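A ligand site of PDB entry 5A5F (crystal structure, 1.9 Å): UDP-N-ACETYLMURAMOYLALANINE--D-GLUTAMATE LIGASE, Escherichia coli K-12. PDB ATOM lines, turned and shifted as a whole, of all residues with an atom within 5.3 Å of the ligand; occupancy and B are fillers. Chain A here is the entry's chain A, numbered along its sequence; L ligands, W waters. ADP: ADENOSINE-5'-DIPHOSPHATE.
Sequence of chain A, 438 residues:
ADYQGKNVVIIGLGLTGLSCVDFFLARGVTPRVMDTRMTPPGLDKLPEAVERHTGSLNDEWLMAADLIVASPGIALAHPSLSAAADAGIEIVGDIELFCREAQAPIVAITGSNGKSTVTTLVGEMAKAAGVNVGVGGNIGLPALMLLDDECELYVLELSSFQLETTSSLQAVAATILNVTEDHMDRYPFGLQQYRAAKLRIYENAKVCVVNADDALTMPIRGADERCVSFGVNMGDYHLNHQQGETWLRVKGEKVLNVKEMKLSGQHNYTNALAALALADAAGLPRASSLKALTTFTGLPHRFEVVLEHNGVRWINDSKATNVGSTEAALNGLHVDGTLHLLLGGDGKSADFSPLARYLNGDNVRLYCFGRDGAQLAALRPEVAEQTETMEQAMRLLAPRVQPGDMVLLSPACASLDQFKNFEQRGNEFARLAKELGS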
ATOM      1  N   GLY A 111      10.901 -24.232   1.333  1.00  0.00           N
ATOM      2  CA  GLY A 111      10.534 -23.935  -0.049  1.00  0.00           C
ATOM      3  C   GLY A 111      10.641 -22.467  -0.357  1.00  0.00           C
ATOM      4  O   GLY A 111      10.782 -21.638   0.531  1.00  0.00           O
ATOM      5  N   SER A 112      10.677 -22.140  -1.638  1.00  0.00           N
ATOM      6  CA  SER A 112      10.876 -20.768  -2.052  1.00  0.00           C
ATOM      7  C   SER A 112       9.646 -19.883  -1.759  1.00  0.00           C
ATOM      8  O   SER A 112       9.807 -18.761  -1.314  1.00  0.00           O
ATOM      9  CB  SER A 112      11.190 -20.747  -3.555  1.00  0.00           C
ATOM     10  OG  SER A 112      12.349 -21.538  -3.770  1.00  0.00           O
ATOM     11  N   ASN A 113       8.438 -20.435  -1.930  1.00  0.00           N
ATOM     12  CA  ASN A 113       7.198 -19.632  -1.740  1.00  0.00           C
ATOM     13  C   ASN A 113       6.041 -20.506  -1.184  1.00  0.00           C
ATOM     14  O   ASN A 113       5.960 -21.728  -1.458  1.00  0.00           O
ATOM     15  CB  ASN A 113       6.714 -18.904  -3.088  1.00  0.00           C
ATOM     16  CG  ASN A 113       7.712 -17.903  -3.665  1.00  0.00           C
ATOM     17  OD1 ASN A 113       8.022 -16.854  -3.054  1.00  0.00           O
ATOM     18  ND2 ASN A 113       8.146 -18.145  -4.921  1.00  0.00           N
ATOM     19  N   GLY A 114       5.126 -19.910  -0.424  1.00  0.00           N
ATOM     20  CA  GLY A 114       4.094 -20.743   0.217  1.00  0.00           C
ATOM     21  C   GLY A 114       4.362 -21.194   1.641  1.00  0.00           C
ATOM     22  O   GLY A 114       3.490 -21.828   2.260  1.00  0.00           O
ATOM     23  N   LYS A 115       5.551 -20.898   2.171  1.00  0.00           N
ATOM     24  CA  LYS A 115       5.944 -21.444   3.496  1.00  0.00           C
ATOM     25  C   LYS A 115       5.017 -20.997   4.610  1.00  0.00           C
ATOM     26  O   LYS A 115       4.536 -21.821   5.374  1.00  0.00           O
ATOM     27  CB  LYS A 115       7.378 -21.079   3.875  1.00  0.00           C
ATOM     28  CG  LYS A 115       8.406 -21.729   2.967  1.00  0.00           C
ATOM     29  CD  LYS A 115       9.835 -21.340   3.320  1.00  0.00           C
ATOM     30  CE  LYS A 115      10.103 -19.826   3.263  1.00  0.00           C
ATOM     31  NZ  LYS A 115      10.013 -19.304   1.889  1.00  0.00           N
ATOM     32  N   SER A 116       4.815 -19.688   4.714  1.00  0.00           N
ATOM     33  CA  SER A 116       3.969 -19.205   5.807  1.00  0.00           C
ATOM     34  C   SER A 116       2.504 -19.657   5.679  1.00  0.00           C
ATOM     35  O   SER A 116       1.808 -19.903   6.687  1.00  0.00           O
ATOM     36  CB  SER A 116       4.052 -17.684   5.842  1.00  0.00           C
ATOM     37  OG  SER A 116       5.332 -17.365   6.337  1.00  0.00           O
ATOM     38  N   THR A 117       1.989 -19.679   4.446  1.00  0.00           N
ATOM     39  CA  THR A 117       0.658 -20.224   4.207  1.00  0.00           C
ATOM     40  C   THR A 117       0.535 -21.636   4.701  1.00  0.00           C
ATOM     41  O   THR A 117      -0.354 -21.946   5.467  1.00  0.00           O
ATOM     42  CB  THR A 117       0.249 -20.152   2.710  1.00  0.00           C
ATOM     43  OG1 THR A 117       0.220 -18.762   2.329  1.00  0.00           O
ATOM     44  CG2 THR A 117      -1.138 -20.714   2.525  1.00  0.00           C
ATOM     45  N   VAL A 118       1.451 -22.496   4.259  1.00  0.00           N
ATOM     46  CA  VAL A 118       1.407 -23.905   4.652  1.00  0.00           C
ATOM     47  C   VAL A 118       1.676 -24.087   6.148  1.00  0.00           C
ATOM     48  O   VAL A 118       0.968 -24.822   6.814  1.00  0.00           O
ATOM     49  CB  VAL A 118       2.321 -24.801   3.769  1.00  0.00           C
ATOM     50  CG1 VAL A 118       2.283 -26.251   4.268  1.00  0.00           C
ATOM     51  CG2 VAL A 118       1.806 -24.770   2.327  1.00  0.00           C
ATOM     52  N   GLU A 157       8.512 -23.322  10.261  1.00  0.00           N
ATOM     53  CA  GLU A 157       8.906 -22.862   8.946  1.00  0.00           C
ATOM     54  C   GLU A 157      10.409 -22.632   8.986  1.00  0.00           C
ATOM     55  O   GLU A 157      10.928 -21.984   9.920  1.00  0.00           O
ATOM     56  CB  GLU A 157       8.178 -21.547   8.634  1.00  0.00           C
ATOM     57  CG  GLU A 157       8.613 -20.939   7.303  1.00  0.00           C
ATOM     58  CD  GLU A 157       7.952 -19.604   7.036  1.00  0.00           C
ATOM     59  OE1 GLU A 157       6.752 -19.411   7.401  1.00  0.00           O
ATOM     60  OE2 GLU A 157       8.599 -18.768   6.386  1.00  0.00           O
ATOM     61  N   LEU A 177       8.284 -27.139  -0.517  1.00  0.00           N
ATOM     62  CA  LEU A 177       7.072 -26.962  -1.266  1.00  0.00           C
ATOM     63  C   LEU A 177       7.386 -26.737  -2.746  1.00  0.00           C
ATOM     64  O   LEU A 177       6.602 -27.173  -3.625  1.00  0.00           O
ATOM     65  CB  LEU A 177       6.299 -25.771  -0.705  1.00  0.00           C
ATOM     66  CG  LEU A 177       5.817 -25.904   0.750  1.00  0.00           C
ATOM     67  CD1 LEU A 177       5.302 -24.521   1.146  1.00  0.00           C
ATOM     68  CD2 LEU A 177       4.694 -26.946   0.799  1.00  0.00           C
ATOM     69  N   ASN A 178       8.541 -26.132  -3.013  1.00  0.00           N
ATOM     70  CA  ASN A 178       8.968 -25.763  -4.373  1.00  0.00           C
ATOM     71  C   ASN A 178      10.355 -25.133  -4.285  1.00  0.00           C
ATOM     72  O   ASN A 178      10.815 -24.720  -3.201  1.00  0.00           O
ATOM     73  CB  ASN A 178       7.976 -24.761  -5.040  1.00  0.00           C
ATOM     74  CG  ASN A 178       7.589 -23.617  -4.097  1.00  0.00           C
ATOM     75  OD1 ASN A 178       8.404 -22.763  -3.802  1.00  0.00           O
ATOM     76  ND2 ASN A 178       6.379 -23.658  -3.562  1.00  0.00           N
ATOM     77  N   HIS A 267      -2.647 -22.885  -6.775  1.00  0.00           N
ATOM     78  CA  HIS A 267      -1.474 -23.111  -5.929  1.00  0.00           C
ATOM     79  C   HIS A 267      -1.787 -23.096  -4.427  1.00  0.00           C
ATOM     80  O   HIS A 267      -1.108 -23.745  -3.655  1.00  0.00           O
ATOM     81  CB  HIS A 267      -0.355 -22.131  -6.253  1.00  0.00           C
ATOM     82  CG  HIS A 267      -0.758 -20.704  -6.114  1.00  0.00           C
ATOM     83  ND1 HIS A 267      -1.862 -20.169  -6.748  1.00  0.00           N
ATOM     84  CD2 HIS A 267      -0.193 -19.683  -5.426  1.00  0.00           C
ATOM     85  CE1 HIS A 267      -1.956 -18.887  -6.474  1.00  0.00           C
ATOM     86  NE2 HIS A 267      -0.949 -18.556  -5.674  1.00  0.00           N
ATOM     87  N   ASN A 268      -2.774 -22.317  -4.009  1.00  0.00           N
ATOM     88  CA  ASN A 268      -3.322 -22.452  -2.633  1.00  0.00           C
ATOM     89  C   ASN A 268      -4.054 -23.795  -2.411  1.00  0.00           C
ATOM     90  O   ASN A 268      -4.027 -24.354  -1.300  1.00  0.00           O
ATOM     91  CB  ASN A 268      -4.259 -21.280  -2.319  1.00  0.00           C
ATOM     92  CG  ASN A 268      -3.472 -20.093  -1.765  1.00  0.00           C
ATOM     93  OD1 ASN A 268      -2.445 -20.290  -1.136  1.00  0.00           O
ATOM     94  ND2 ASN A 268      -3.930 -18.873  -2.037  1.00  0.00           N
ATOM     95  N   THR A 270      -3.074 -26.623  -3.877  1.00  0.00           N
ATOM     96  CA  THR A 270      -1.951 -27.536  -3.607  1.00  0.00           C
ATOM     97  C   THR A 270      -1.279 -27.248  -2.243  1.00  0.00           C
ATOM     98  O   THR A 270      -0.836 -28.178  -1.584  1.00  0.00           O
ATOM     99  CB  THR A 270      -0.917 -27.637  -4.752  1.00  0.00           C
ATOM    100  OG1 THR A 270      -0.331 -26.366  -5.000  1.00  0.00           O
ATOM    101  CG2 THR A 270      -1.568 -28.124  -6.051  1.00  0.00           C
ATOM    102  N   ASN A 271      -1.211 -25.979  -1.819  1.00  0.00           N
ATOM    103  CA  ASN A 271      -0.755 -25.714  -0.438  1.00  0.00           C
ATOM    104  C   ASN A 271      -1.610 -26.473   0.597  1.00  0.00           C
ATOM    105  O   ASN A 271      -1.069 -26.994   1.599  1.00  0.00           O
ATOM    106  CB  ASN A 271      -0.810 -24.195  -0.095  1.00  0.00           C
ATOM    107  CG  ASN A 271       0.268 -23.380  -0.812  1.00  0.00           C
ATOM    108  OD1 ASN A 271       1.296 -23.918  -1.259  1.00  0.00           O
ATOM    109  ND2 ASN A 271       0.035 -22.060  -0.947  1.00  0.00           N
ATOM    110  N   LEU A 299      -3.564 -15.882   4.416  1.00  0.00           N
ATOM    111  CA  LEU A 299      -2.810 -14.744   4.945  1.00  0.00           C
ATOM    112  C   LEU A 299      -3.070 -13.531   4.041  1.00  0.00           C
ATOM    113  O   LEU A 299      -3.441 -13.664   2.864  1.00  0.00           O
ATOM    114  CB  LEU A 299      -1.326 -15.108   4.927  1.00  0.00           C
ATOM    115  CG  LEU A 299      -1.011 -16.260   5.893  1.00  0.00           C
ATOM    116  CD1 LEU A 299       0.461 -16.600   5.842  1.00  0.00           C
ATOM    117  CD2 LEU A 299      -1.430 -15.915   7.313  1.00  0.00           C
ATOM    118  N   HIS A 301      -2.881 -10.603   1.475  1.00  0.00           N
ATOM    119  CA  HIS A 301      -2.003 -10.286   0.331  1.00  0.00           C
ATOM    120  C   HIS A 301      -1.420 -11.505  -0.410  1.00  0.00           C
ATOM    121  O   HIS A 301      -0.543 -11.361  -1.295  1.00  0.00           O
ATOM    122  CB  HIS A 301      -0.827  -9.412   0.782  1.00  0.00           C
ATOM    123  CG  HIS A 301      -1.239  -8.216   1.562  1.00  0.00           C
ATOM    124  ND1 HIS A 301      -1.051  -8.109   2.926  1.00  0.00           N
ATOM    125  CD2 HIS A 301      -1.879  -7.087   1.179  1.00  0.00           C
ATOM    126  CE1 HIS A 301      -1.558  -6.964   3.353  1.00  0.00           C
ATOM    127  NE2 HIS A 301      -2.048  -6.306   2.305  1.00  0.00           N
ATOM    128  N   ARG A 302      -1.857 -12.688  -0.042  1.00  0.00           N
ATOM    129  CA  ARG A 302      -1.381 -13.904  -0.676  1.00  0.00           C
ATOM    130  C   ARG A 302      -2.499 -14.375  -1.567  1.00  0.00           C
ATOM    131  O   ARG A 302      -3.431 -15.047  -1.083  1.00  0.00           O
ATOM    132  CB  ARG A 302      -1.098 -14.995   0.365  1.00  0.00           C
ATOM    133  CG  ARG A 302       0.256 -14.961   1.034  1.00  0.00           C
ATOM    134  CD  ARG A 302       0.407 -13.817   2.034  1.00  0.00           C
ATOM    135  NE  ARG A 302       1.556 -14.015   2.930  1.00  0.00           N
ATOM    136  CZ  ARG A 302       1.808 -13.257   3.999  1.00  0.00           C
ATOM    137  NH1 ARG A 302       1.015 -12.242   4.336  1.00  0.00           N
ATOM    138  NH2 ARG A 302       2.881 -13.507   4.746  1.00  0.00           N
ATOM    139  N   PHE A 303      -2.421 -14.059  -2.853  1.00  0.00           N
ATOM    140  CA  PHE A 303      -3.539 -14.356  -3.770  1.00  0.00           C
ATOM    141  C   PHE A 303      -4.910 -14.251  -3.039  1.00  0.00           C
ATOM    142  O   PHE A 303      -5.723 -15.192  -3.012  1.00  0.00           O
ATOM    143  CB  PHE A 303      -3.341 -15.750  -4.378  1.00  0.00           C
ATOM    144  CG  PHE A 303      -4.049 -15.938  -5.708  1.00  0.00           C
ATOM    145  CD1 PHE A 303      -3.465 -15.481  -6.876  1.00  0.00           C
ATOM    146  CD2 PHE A 303      -5.283 -16.547  -5.764  1.00  0.00           C
ATOM    147  CE1 PHE A 303      -4.088 -15.675  -8.105  1.00  0.00           C
ATOM    148  CE2 PHE A 303      -5.914 -16.743  -6.981  1.00  0.00           C
ATOM    149  CZ  PHE A 303      -5.319 -16.278  -8.148  1.00  0.00           C
ATOM    150  N   ASP A 317      -2.637 -10.092  -4.814  1.00  0.00           N
ATOM    151  CA  ASP A 317      -1.472 -10.950  -4.629  1.00  0.00           C
ATOM    152  C   ASP A 317      -0.247 -10.040  -4.521  1.00  0.00           C
ATOM    153  O   ASP A 317       0.811 -10.325  -5.047  1.00  0.00           O
ATOM    154  CB  ASP A 317      -1.340 -11.964  -5.795  1.00  0.00           C
ATOM    155  CG  ASP A 317      -0.345 -13.104  -5.481  1.00  0.00           C
ATOM    156  OD1 ASP A 317      -0.179 -13.448  -4.298  1.00  0.00           O
ATOM    157  OD2 ASP A 317       0.266 -13.668  -6.435  1.00  0.00           O
ATOM    158  N   LYS A 319       1.787  -9.782  -2.106  1.00  0.00           N
ATOM    159  CA  LYS A 319       2.942 -10.480  -1.577  1.00  0.00           C
ATOM    160  C   LYS A 319       3.819 -11.156  -2.651  1.00  0.00           C
ATOM    161  O   LYS A 319       4.909 -11.674  -2.359  1.00  0.00           O
ATOM    162  CB  LYS A 319       2.546 -11.447  -0.455  1.00  0.00           C
ATOM    163  CG  LYS A 319       3.702 -12.210   0.154  1.00  0.00           C
ATOM    164  CD  LYS A 319       4.410 -11.408   1.223  1.00  0.00           C
ATOM    165  CE  LYS A 319       5.691 -12.059   1.722  1.00  0.00           C
ATOM    166  NZ  LYS A 319       5.394 -13.263   2.547  1.00  0.00           N
ATOM    167  N   ALA A 320       3.350 -11.167  -3.892  1.00  0.00           N
ATOM    168  CA  ALA A 320       4.153 -11.785  -4.950  1.00  0.00           C
ATOM    169  C   ALA A 320       5.230 -10.788  -5.448  1.00  0.00           C
ATOM    170  O   ALA A 320       5.029 -10.029  -6.409  1.00  0.00           O
ATOM    171  CB  ALA A 320       3.238 -12.287  -6.086  1.00  0.00           C
ATOM    172  N   GLY A 324       8.801 -16.225  -9.133  1.00  0.00           N
ATOM    173  CA  GLY A 324       8.269 -17.566  -8.810  1.00  0.00           C
ATOM    174  C   GLY A 324       6.814 -17.543  -8.283  1.00  0.00           C
ATOM    175  O   GLY A 324       5.964 -18.385  -8.648  1.00  0.00           O
ATOM    176  N   SER A 325       6.510 -16.561  -7.437  1.00  0.00           N
ATOM    177  CA  SER A 325       5.163 -16.369  -6.898  1.00  0.00           C
ATOM    178  C   SER A 325       4.146 -16.025  -7.992  1.00  0.00           C
ATOM    179  O   SER A 325       3.067 -16.560  -8.051  1.00  0.00           O
ATOM    180  CB  SER A 325       5.172 -15.157  -5.942  1.00  0.00           C
ATOM    181  OG  SER A 325       5.822 -15.513  -4.765  1.00  0.00           O
ATOM    182  N   ALA A 328       3.499 -18.904 -10.331  1.00  0.00           N
ATOM    183  CA  ALA A 328       2.629 -19.932  -9.758  1.00  0.00           C
ATOM    184  C   ALA A 328       1.189 -19.440  -9.892  1.00  0.00           C
ATOM    185  O   ALA A 328       0.297 -20.209 -10.232  1.00  0.00           O
ATOM    186  CB  ALA A 328       2.983 -20.163  -8.276  1.00  0.00           C
HETATM  187  PB  ADP L   1       6.552 -17.471   2.022  1.00  0.00           P
HETATM  188  O1B ADP L   1       7.084 -16.114   1.684  1.00  0.00           O
HETATM  189  O2B ADP L   1       7.330 -18.638   1.505  1.00  0.00           O
HETATM  190  O3B ADP L   1       6.270 -17.630   3.511  1.00  0.00           O
HETATM  191  PA  ADP L   1       3.672 -17.068   1.524  1.00  0.00           P
HETATM  192  O1A ADP L   1       2.736 -18.128   1.904  1.00  0.00           O
HETATM  193  O2A ADP L   1       3.814 -15.760   2.328  1.00  0.00           O
HETATM  194  O3A ADP L   1       5.140 -17.684   1.325  1.00  0.00           O
HETATM  195  O5' ADP L   1       3.369 -16.606  -0.016  1.00  0.00           O
HETATM  196  C5' ADP L   1       4.266 -15.649  -0.643  1.00  0.00           C
HETATM  197  C4' ADP L   1       3.891 -15.411  -2.131  1.00  0.00           C
HETATM  198  O4' ADP L   1       3.926 -16.670  -2.835  1.00  0.00           O
HETATM  199  C3' ADP L   1       2.428 -14.917  -2.300  1.00  0.00           C
HETATM  200  O3' ADP L   1       2.343 -14.184  -3.527  1.00  0.00           O
HETATM  201  C2' ADP L   1       1.691 -16.239  -2.513  1.00  0.00           C
HETATM  202  O2' ADP L   1       0.422 -16.133  -3.173  1.00  0.00           O
HETATM  203  C1' ADP L   1       2.660 -17.040  -3.382  1.00  0.00           C
HETATM  204  N9  ADP L   1       2.531 -18.519  -3.175  1.00  0.00           N
HETATM  205  C8  ADP L   1       1.835 -19.147  -2.194  1.00  0.00           C
HETATM  206  N7  ADP L   1       1.983 -20.471  -2.261  1.00  0.00           N
HETATM  207  C5  ADP L   1       2.767 -20.697  -3.332  1.00  0.00           C
HETATM  208  C6  ADP L   1       3.319 -21.871  -3.982  1.00  0.00           C
HETATM  209  N6  ADP L   1       3.027 -23.083  -3.460  1.00  0.00           N
HETATM  210  N1  ADP L   1       4.086 -21.668  -5.068  1.00  0.00           N
HETATM  211  C2  ADP L   1       4.412 -20.450  -5.553  1.00  0.00           C
HETATM  212  N3  ADP L   1       3.934 -19.316  -5.015  1.00  0.00           N
HETATM  213  C4  ADP L   1       3.143 -19.408  -3.912  1.00  0.00           C
HETATM  214  O   HOH W   1       0.943 -16.186  -6.108  1.00  0.00           O
HETATM  215  O   HOH W   2       4.239 -25.665  -4.073  1.00  0.00           O
HETATM  216  O   HOH W   3       9.751 -16.339   3.067  1.00  0.00           O
HETATM  217  O   HOH W   4       7.725 -15.543  -0.766  1.00  0.00           O
HETATM  218  O   HOH W   5       4.720 -23.461  -6.938  1.00  0.00           O
HETATM  219  O   HOH W   6       1.633 -26.074  -2.985  1.00  0.00           O
HETATM  220  O   HOH W   7      -0.603 -18.430  -0.375  1.00  0.00           O
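The side-chain carboxylate of Asp 317 is in hydrogen-bond range of the backbone NH of Phe 303 (2.7 Å). O of Ser 112 sits at hydrogen-bond distance from NZ of Lys 115 (3.3 Å). The side-chain amino group of Lys 115 is in hydrogen-bond range of the backbone carbonyl oxygen of Gly 111 (2.8 Å). The side-chain amide nitrogen of Asn 271 sits at hydrogen-bond distance from the side-chain amide oxygen of Asn 268 (3.1 Å). The side-chain hydroxyl of Ser 325 is in hydrogen-bond range of the side-chain amide oxygen of Asn 113 (3.1 Å). The side-chain amide nitrogen (ND2) of Asn 178 is in hydrogen-bond range of the backbone carbonyl oxygen (O) of Asn 113, 2.9 Å away. O of Asn 178 is in hydrogen-bond range of N of Ser 112 (3.0 Å). O of His 267 is in hydrogen-bond range of OG1 of Thr 270 (3.0 Å).
Water W4 bridges an oxygen (O1B) of the ligand and the side-chain amide oxygen (OD1) of Asn 113. Water W2 lies within hydrogen-bond range of O of Leu 177 (2.8 Å), N6 of the ligand (2.9 Å) and ND2 of Asn 178 (3.0 Å). Water W1 lies within hydrogen-bond range of OD2 of Asp 317 (2.6 Å), O of Ser 325 (2.9 Å), O2' of the ligand (3.0 Å) and NE2 of His 267 (3.1 Å). Water W3 lies within hydrogen-bond range of O1B of the ligand (3.0 Å) and NZ of Lys 115 (3.2 Å). Water W7 lies within hydrogen-bond range of the side-chain amide oxygen (OD1) of Asn 268 (2.7 Å) and the side-chain hydroxyl (OG1) of Thr 117 (2.8 Å). Water W6 lies within hydrogen-bond range of the side-chain amide oxygen of Asn 271 (2.8 Å), the side-chain hydroxyl of Thr 270 (2.8 Å) and a nitrogen (N6) of the ligand (3.3 Å).
O of Ser 112 touches O2B of the ligand, at 3.8 Å. CA of Asn 113 touches O2B of the ligand, 3.4 Å away. Glu 157 touches the ligand (OE2 to O3B, 3.9 Å). CD2 of His 267 touches C4 of the ligand (3.7 Å). Phe 303 touches the ligand (N to O2', 3.5 Å). Ala 328 touches the ligand (CB to C2, 3.1 Å). Of the 25 residues printed, 17 come within 4 Å of the ligand.
N of Thr 117 lies within hydrogen-bond range of O1A of the ligand (3.1 Å). The side-chain hydroxyl (OG1) of Thr 117 lies within hydrogen-bond range of an oxygen (O1A) of the ligand, 2.6 Å away. OD1 of Asp 317 sits at hydrogen-bond distance from O3' of the ligand, 2.7 Å away. An oxygen (O2B) of the ligand sits at hydrogen-bond distance from the backbone NH (N) of Lys 115. O2B of the ligand lies within salt-bridge range of NZ of Lys 115 (2.8 Å). N of Ser 116 is in hydrogen-bond range of O3B of the ligand (2.8 Å). OG of Ser 116 lies within hydrogen-bond range of O3B of the ligand, at 3.0 Å. The backbone NH of Gly 114 lies within hydrogen-bond range of an oxygen (O3A) of the ligand. ND2 of Asn 271 lies within hydrogen-bond range of N7 of the ligand (2.8 Å). NE of Arg 302 lies within salt-bridge range of O2A of the ligand (2.9 Å). An oxygen (O4') of the ligand sits at hydrogen-bond distance from the side-chain hydroxyl of Ser 325. The side-chain amino group (NZ) of Lys 319 lies within salt-bridge range of an oxygen (O2A) of the ligand, 3.0 Å away. An oxygen (O3') of the ligand lies within hydrogen-bond range of the backbone NH of Ala 320, at 3.2 Å. The side-chain amide nitrogen of Asn 178 lies within hydrogen-bond range of a nitrogen (N1) of the ligand (3.4 Å).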
